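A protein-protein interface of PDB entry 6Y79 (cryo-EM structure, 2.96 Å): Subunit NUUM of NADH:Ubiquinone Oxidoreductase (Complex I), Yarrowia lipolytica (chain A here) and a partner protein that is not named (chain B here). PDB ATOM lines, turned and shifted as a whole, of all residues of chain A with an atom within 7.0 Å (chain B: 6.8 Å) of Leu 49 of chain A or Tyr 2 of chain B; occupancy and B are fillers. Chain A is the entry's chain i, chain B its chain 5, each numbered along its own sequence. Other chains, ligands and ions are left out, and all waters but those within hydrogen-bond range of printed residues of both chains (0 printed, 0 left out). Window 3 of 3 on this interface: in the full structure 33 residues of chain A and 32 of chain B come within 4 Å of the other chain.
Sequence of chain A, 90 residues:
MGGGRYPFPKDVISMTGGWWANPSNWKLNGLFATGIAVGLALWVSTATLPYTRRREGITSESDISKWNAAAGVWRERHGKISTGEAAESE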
ATOM      1  N   LEU A  42      14.873  12.287 -18.610  1.00  0.00           N
ATOM      2  CA  LEU A  42      14.383  13.635 -18.324  1.00  0.00           C
ATOM      3  C   LEU A  42      14.025  14.382 -19.601  1.00  0.00           C
ATOM      4  O   LEU A  42      12.997  15.071 -19.664  1.00  0.00           O
ATOM      5  CB  LEU A  42      15.447  14.424 -17.561  1.00  0.00           C
ATOM      6  CG  LEU A  42      15.736  14.225 -16.071  1.00  0.00           C
ATOM      7  CD1 LEU A  42      17.012  14.977 -15.708  1.00  0.00           C
ATOM      8  CD2 LEU A  42      14.578  14.630 -15.184  1.00  0.00           C
ATOM      9  N   VAL A  44      13.308  13.164 -22.752  1.00  0.00           N
ATOM     10  CA  VAL A  44      12.123  12.581 -23.381  1.00  0.00           C
ATOM     11  C   VAL A  44      10.880  12.887 -22.554  1.00  0.00           C
ATOM     12  O   VAL A  44       9.800  13.132 -23.113  1.00  0.00           O
ATOM     13  CB  VAL A  44      12.329  11.064 -23.590  1.00  0.00           C
ATOM     14  CG1 VAL A  44      11.053  10.370 -24.028  1.00  0.00           C
ATOM     15  CG2 VAL A  44      13.403  10.817 -24.627  1.00  0.00           C
ATOM     16  N   SER A  45      11.027  12.938 -21.223  1.00  0.00           N
ATOM     17  CA  SER A  45       9.917  13.279 -20.342  1.00  0.00           C
ATOM     18  C   SER A  45       9.383  14.681 -20.622  1.00  0.00           C
ATOM     19  O   SER A  45       8.172  14.867 -20.767  1.00  0.00           O
ATOM     20  CB  SER A  45      10.363  13.153 -18.889  1.00  0.00           C
ATOM     21  OG  SER A  45       9.276  13.292 -18.002  1.00  0.00           O
ATOM     22  N   THR A  46      10.263  15.675 -20.743  1.00  0.00           N
ATOM     23  CA  THR A  46       9.757  17.028 -20.986  1.00  0.00           C
ATOM     24  C   THR A  46       9.413  17.282 -22.451  1.00  0.00           C
ATOM     25  O   THR A  46       8.606  18.173 -22.736  1.00  0.00           O
ATOM     26  CB  THR A  46      10.749  18.082 -20.501  1.00  0.00           C
ATOM     27  OG1 THR A  46      11.856  18.156 -21.403  1.00  0.00           O
ATOM     28  CG2 THR A  46      11.214  17.770 -19.099  1.00  0.00           C
ATOM     29  N   ALA A  47      10.004  16.533 -23.385  1.00  0.00           N
ATOM     30  CA  ALA A  47       9.750  16.794 -24.800  1.00  0.00           C
ATOM     31  C   ALA A  47       8.359  16.337 -25.221  1.00  0.00           C
ATOM     32  O   ALA A  47       7.742  16.943 -26.104  1.00  0.00           O
ATOM     33  CB  ALA A  47      10.811  16.112 -25.653  1.00  0.00           C
ATOM     34  N   THR A  48       7.847  15.273 -24.614  1.00  0.00           N
ATOM     35  CA  THR A  48       6.537  14.754 -24.968  1.00  0.00           C
ATOM     36  C   THR A  48       5.427  15.304 -24.090  1.00  0.00           C
ATOM     37  O   THR A  48       4.335  14.731 -24.074  1.00  0.00           O
ATOM     38  CB  THR A  48       6.539  13.230 -24.892  1.00  0.00           C
ATOM     39  OG1 THR A  48       6.880  12.832 -23.564  1.00  0.00           O
ATOM     40  CG2 THR A  48       7.549  12.654 -25.858  1.00  0.00           C
ATOM     41  N   LEU A  49       5.685  16.392 -23.352  1.00  0.00           N
ATOM     42  CA  LEU A  49       4.646  16.975 -22.501  1.00  0.00           C
ATOM     43  C   LEU A  49       3.468  17.572 -23.272  1.00  0.00           C
ATOM     44  O   LEU A  49       2.322  17.227 -22.934  1.00  0.00           O
ATOM     45  CB  LEU A  49       5.264  17.996 -21.538  1.00  0.00           C
ATOM     46  CG  LEU A  49       6.055  17.578 -20.304  1.00  0.00           C
ATOM     47  CD1 LEU A  49       6.713  18.799 -19.706  1.00  0.00           C
ATOM     48  CD2 LEU A  49       5.146  16.937 -19.287  1.00  0.00           C
ATOM     49  N   PRO A  50       3.636  18.454 -24.278  1.00  0.00           N
ATOM     50  CA  PRO A  50       2.437  19.027 -24.917  1.00  0.00           C
ATOM     51  C   PRO A  50       1.707  18.069 -25.830  1.00  0.00           C
ATOM     52  O   PRO A  50       0.591  18.380 -26.264  1.00  0.00           O
ATOM     53  CB  PRO A  50       2.996  20.203 -25.715  1.00  0.00           C
ATOM     54  CG  PRO A  50       4.312  19.739 -26.109  1.00  0.00           C
ATOM     55  CD  PRO A  50       4.841  19.057 -24.897  1.00  0.00           C
ATOM     56  N   TYR A  51       2.294  16.923 -26.137  1.00  0.00           N
ATOM     57  CA  TYR A  51       1.620  15.899 -26.909  1.00  0.00           C
ATOM     58  C   TYR A  51       0.708  15.035 -26.058  1.00  0.00           C
ATOM     59  O   TYR A  51       0.049  14.140 -26.594  1.00  0.00           O
ATOM     60  CB  TYR A  51       2.668  15.060 -27.623  1.00  0.00           C
ATOM     61  CG  TYR A  51       3.459  15.888 -28.602  1.00  0.00           C
ATOM     62  CD1 TYR A  51       2.931  16.213 -29.845  1.00  0.00           C
ATOM     63  CD2 TYR A  51       4.715  16.377 -28.273  1.00  0.00           C
ATOM     64  CE1 TYR A  51       3.639  16.984 -30.736  1.00  0.00           C
ATOM     65  CE2 TYR A  51       5.429  17.147 -29.156  1.00  0.00           C
ATOM     66  CZ  TYR A  51       4.886  17.448 -30.385  1.00  0.00           C
ATOM     67  OH  TYR A  51       5.600  18.222 -31.266  1.00  0.00           O
ATOM     68  N   THR A  52       0.644  15.295 -24.755  1.00  0.00           N
ATOM     69  CA  THR A  52      -0.279  14.608 -23.873  1.00  0.00           C
ATOM     70  C   THR A  52      -1.582  15.375 -23.737  1.00  0.00           C
ATOM     71  O   THR A  52      -1.593  16.605 -23.668  1.00  0.00           O
ATOM     72  CB  THR A  52       0.320  14.411 -22.486  1.00  0.00           C
ATOM     73  OG1 THR A  52       0.527  15.689 -21.880  1.00  0.00           O
ATOM     74  CG2 THR A  52       1.626  13.694 -22.585  1.00  0.00           C
ATOM     75  N   ARG A  53      -2.681  14.633 -23.686  1.00  0.00           N
ATOM     76  CA  ARG A  53      -3.983  15.209 -23.411  1.00  0.00           C
ATOM     77  C   ARG A  53      -4.788  14.190 -22.627  1.00  0.00           C
ATOM     78  O   ARG A  53      -4.437  13.012 -22.564  1.00  0.00           O
ATOM     79  CB  ARG A  53      -4.705  15.616 -24.700  1.00  0.00           C
ATOM     80  CG  ARG A  53      -5.123  14.451 -25.562  1.00  0.00           C
ATOM     81  CD  ARG A  53      -5.906  14.906 -26.770  1.00  0.00           C
ATOM     82  NE  ARG A  53      -6.198  13.795 -27.668  1.00  0.00           N
ATOM     83  CZ  ARG A  53      -7.249  12.993 -27.545  1.00  0.00           C
ATOM     84  NH1 ARG A  53      -7.433  12.007 -28.409  1.00  0.00           N
ATOM     85  NH2 ARG A  53      -8.116  13.179 -26.562  1.00  0.00           N
ATOM     86  N   TYR B   2       8.369  16.353 -15.704  1.00  0.00           N
ATOM     87  CA  TYR B   2       7.924  15.047 -15.233  1.00  0.00           C
ATOM     88  C   TYR B   2       6.643  14.622 -15.944  1.00  0.00           C
ATOM     89  O   TYR B   2       5.626  15.308 -15.870  1.00  0.00           O
ATOM     90  CB  TYR B   2       7.706  15.074 -13.721  1.00  0.00           C
ATOM     91  CG  TYR B   2       7.309  13.741 -13.142  1.00  0.00           C
ATOM     92  CD1 TYR B   2       8.256  12.757 -12.910  1.00  0.00           C
ATOM     93  CD2 TYR B   2       5.983  13.466 -12.825  1.00  0.00           C
ATOM     94  CE1 TYR B   2       7.896  11.532 -12.379  1.00  0.00           C
ATOM     95  CE2 TYR B   2       5.613  12.245 -12.301  1.00  0.00           C
ATOM     96  CZ  TYR B   2       6.571  11.282 -12.081  1.00  0.00           C
ATOM     97  OH  TYR B   2       6.204  10.068 -11.554  1.00  0.00           O
ATOM     98  N   ASN B   3       6.691  13.473 -16.615  1.00  0.00           N
ATOM     99  CA  ASN B   3       5.587  13.007 -17.450  1.00  0.00           C
ATOM    100  C   ASN B   3       5.396  11.517 -17.218  1.00  0.00           C
ATOM    101  O   ASN B   3       6.220  10.717 -17.664  1.00  0.00           O
ATOM    102  CB  ASN B   3       5.865  13.287 -18.923  1.00  0.00           C
ATOM    103  CG  ASN B   3       4.629  13.179 -19.772  1.00  0.00           C
ATOM    104  OD1 ASN B   3       3.519  13.085 -19.256  1.00  0.00           O
ATOM    105  ND2 ASN B   3       4.809  13.198 -21.084  1.00  0.00           N
ATOM    106  N   ALA B   4       4.296  11.144 -16.560  1.00  0.00           N
ATOM    107  CA  ALA B   4       4.114   9.757 -16.142  1.00  0.00           C
ATOM    108  C   ALA B   4       3.849   8.836 -17.327  1.00  0.00           C
ATOM    109  O   ALA B   4       4.354   7.712 -17.362  1.00  0.00           O
ATOM    110  CB  ALA B   4       2.978   9.662 -15.127  1.00  0.00           C
ATOM    111  N   SER B   6       5.034   9.123 -20.252  1.00  0.00           N
ATOM    112  CA  SER B   6       6.225   9.016 -21.078  1.00  0.00           C
ATOM    113  C   SER B   6       7.325   8.196 -20.434  1.00  0.00           C
ATOM    114  O   SER B   6       8.094   7.545 -21.148  1.00  0.00           O
ATOM    115  CB  SER B   6       6.767  10.407 -21.389  1.00  0.00           C
ATOM    116  OG  SER B   6       7.883  10.325 -22.252  1.00  0.00           O
ATOM    117  N   LEU B   7       7.427   8.225 -19.105  1.00  0.00           N
ATOM    118  CA  LEU B   7       8.486   7.491 -18.427  1.00  0.00           C
ATOM    119  C   LEU B   7       8.253   5.990 -18.480  1.00  0.00           C
ATOM    120  O   LEU B   7       9.223   5.228 -18.578  1.00  0.00           O
ATOM    121  CB  LEU B   7       8.606   7.960 -16.981  1.00  0.00           C
ATOM    122  CG  LEU B   7       9.074   9.403 -16.801  1.00  0.00           C
ATOM    123  CD1 LEU B   7       9.054   9.785 -15.341  1.00  0.00           C
ATOM    124  CD2 LEU B   7      10.442   9.618 -17.400  1.00  0.00           C
ATOM    125  N   LEU B  44       7.489   1.633  -9.822  1.00  0.00           N
ATOM    126  CA  LEU B  44       7.029   2.593  -8.821  1.00  0.00           C
ATOM    127  C   LEU B  44       6.194   3.698  -9.460  1.00  0.00           C
ATOM    128  O   LEU B  44       5.154   4.101  -8.909  1.00  0.00           O
ATOM    129  CB  LEU B  44       8.219   3.179  -8.066  1.00  0.00           C
ATOM    130  CG  LEU B  44       8.917   2.222  -7.100  1.00  0.00           C
ATOM    131  CD1 LEU B  44      10.128   2.881  -6.479  1.00  0.00           C
ATOM    132  CD2 LEU B  44       7.958   1.750  -6.029  1.00  0.00           C
ATOM    133  N   ILE B  45       6.612   4.160 -10.647  1.00  0.00           N
ATOM    134  CA  ILE B  45       5.842   5.160 -11.388  1.00  0.00           C
ATOM    135  C   ILE B  45       4.469   4.614 -11.781  1.00  0.00           C
ATOM    136  O   ILE B  45       3.457   5.320 -11.677  1.00  0.00           O
ATOM    137  CB  ILE B  45       6.646   5.644 -12.612  1.00  0.00           C
ATOM    138  CG1 ILE B  45       7.843   6.477 -12.164  1.00  0.00           C
ATOM    139  CG2 ILE B  45       5.810   6.495 -13.536  1.00  0.00           C
ATOM    140  CD1 ILE B  45       8.889   6.637 -13.235  1.00  0.00           C
ATOM    141  N   TYR B  48       2.129   4.521  -8.749  1.00  0.00           N
ATOM    142  CA  TYR B  48       1.666   5.875  -8.464  1.00  0.00           C
ATOM    143  C   TYR B  48       0.617   6.344  -9.464  1.00  0.00           C
ATOM    144  O   TYR B  48      -0.358   7.000  -9.081  1.00  0.00           O
ATOM    145  CB  TYR B  48       2.856   6.824  -8.461  1.00  0.00           C
ATOM    146  CG  TYR B  48       2.527   8.232  -8.052  1.00  0.00           C
ATOM    147  CD1 TYR B  48       2.202   8.535  -6.739  1.00  0.00           C
ATOM    148  CD2 TYR B  48       2.560   9.265  -8.977  1.00  0.00           C
ATOM    149  CE1 TYR B  48       1.910   9.827  -6.360  1.00  0.00           C
ATOM    150  CE2 TYR B  48       2.270  10.559  -8.608  1.00  0.00           C
ATOM    151  CZ  TYR B  48       1.948  10.833  -7.299  1.00  0.00           C
ATOM    152  OH  TYR B  48       1.657  12.124  -6.932  1.00  0.00           O
ATOM    153  N   LEU B  62      -0.358  10.072 -25.057  1.00  0.00           N
ATOM    154  CA  LEU B  62       0.583  10.900 -25.783  1.00  0.00           C
ATOM    155  C   LEU B  62       0.560  10.544 -27.262  1.00  0.00           C
ATOM    156  O   LEU B  62       0.378   9.384 -27.646  1.00  0.00           O
ATOM    157  CB  LEU B  62       2.006  10.804 -25.206  1.00  0.00           C
ATOM    158  CG  LEU B  62       2.758   9.522 -24.849  1.00  0.00           C
ATOM    159  CD1 LEU B  62       3.349   8.822 -26.071  1.00  0.00           C
ATOM    160  CD2 LEU B  62       3.891   9.917 -23.923  1.00  0.00           C
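The side-chain hydroxyl (OG) of Ser 45 of chain A is in hydrogen-bond range of the backbone NH (N) of Asn 3 of chain B, 2.9 Å away.
OG1 of Thr 48 of chain A is in hydrogen-bond range of ND2 of Asn 3 of chain B, at 3.3 Å.
The side-chain hydroxyl (OG1) of Thr 48 of chain A sits at hydrogen-bond distance from the side-chain hydroxyl (OG) of Ser 6 of chain B, 3.0 Å away.
OG1 of Thr 48 of chain A is in hydrogen-bond range of O of Val 44 of chain A (3.0 Å).
The backbone carbonyl oxygen of Leu 49 of chain A lies within hydrogen-bond range of the side-chain hydroxyl of Thr 52 of chain A, at 2.6 Å.
Among the printed residues, pairs that only touch across the chains: Tyr 51 of chain A with Leu 62 of chain B (3.4 Å), Val 44 of chain A with Ser 6 of chain B (3.5 Å), Ser 45 of chain A with Tyr 2 of chain B (3.5 Å), Thr 52 of chain A with Asn 3 of chain B (3.6 Å), Leu 49 of chain A with Asn 3 of chain B (3.7 Å), Leu 49 of chain A with Tyr 2 of chain B (3.8 Å), Ser 45 of chain A with Leu 7 of chain B (3.8 Å) and Thr 52 of chain A with Leu 62 of chain B (3.9 Å).
Of chain B, only Tyr 2 (3.8 Å) and Asn 3 (3.7 Å) come within 4 Å of Leu 49 of chain A.
Of the printed residues of chain B, Tyr 51 of chain A touches Leu 62 (3.4 Å).
Printed residues of chain B within 4 Å of Thr 52 of chain A: Asn 3 and Leu 62.
Of the printed residues of chain A, Ser 6 of chain B touches Val 44 and Thr 48.
Ile 45 of chain B touches none of the printed residues of chain A.
Pro 50 of chain A touches none of the printed residues of chain B.
The nearest residue of chain A that does not touch Tyr 2 of chain B is Thr 46 of chain A (4.7 Å).
The nearest printed residue of chain A that does not touch Asn 3 of chain B is Thr 46 of chain A (5.3 Å).
Of the 9 printed residues of chain B, 5 touch a printed residue of chain A.
Hydrophobic or aromatic side chains of chain B that line the printed part of chain A: Leu 7 and Leu 62.
Of the 11 printed residues of chain A, 6 touch a printed residue of chain B.
Hydrophobic or aromatic side chains of chain A that line the printed part of chain B: Val 44 and Leu 49.
Along chain A the printed residues that touch a printed residue of chain B span positions 44 to 52.
Among the printed residues, 11 pairs touch across the chains.
Among the printed residues, no Asp or Glu carboxylate lies within 4 Å of a Lys or Arg side-chain nitrogen of the other chain.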
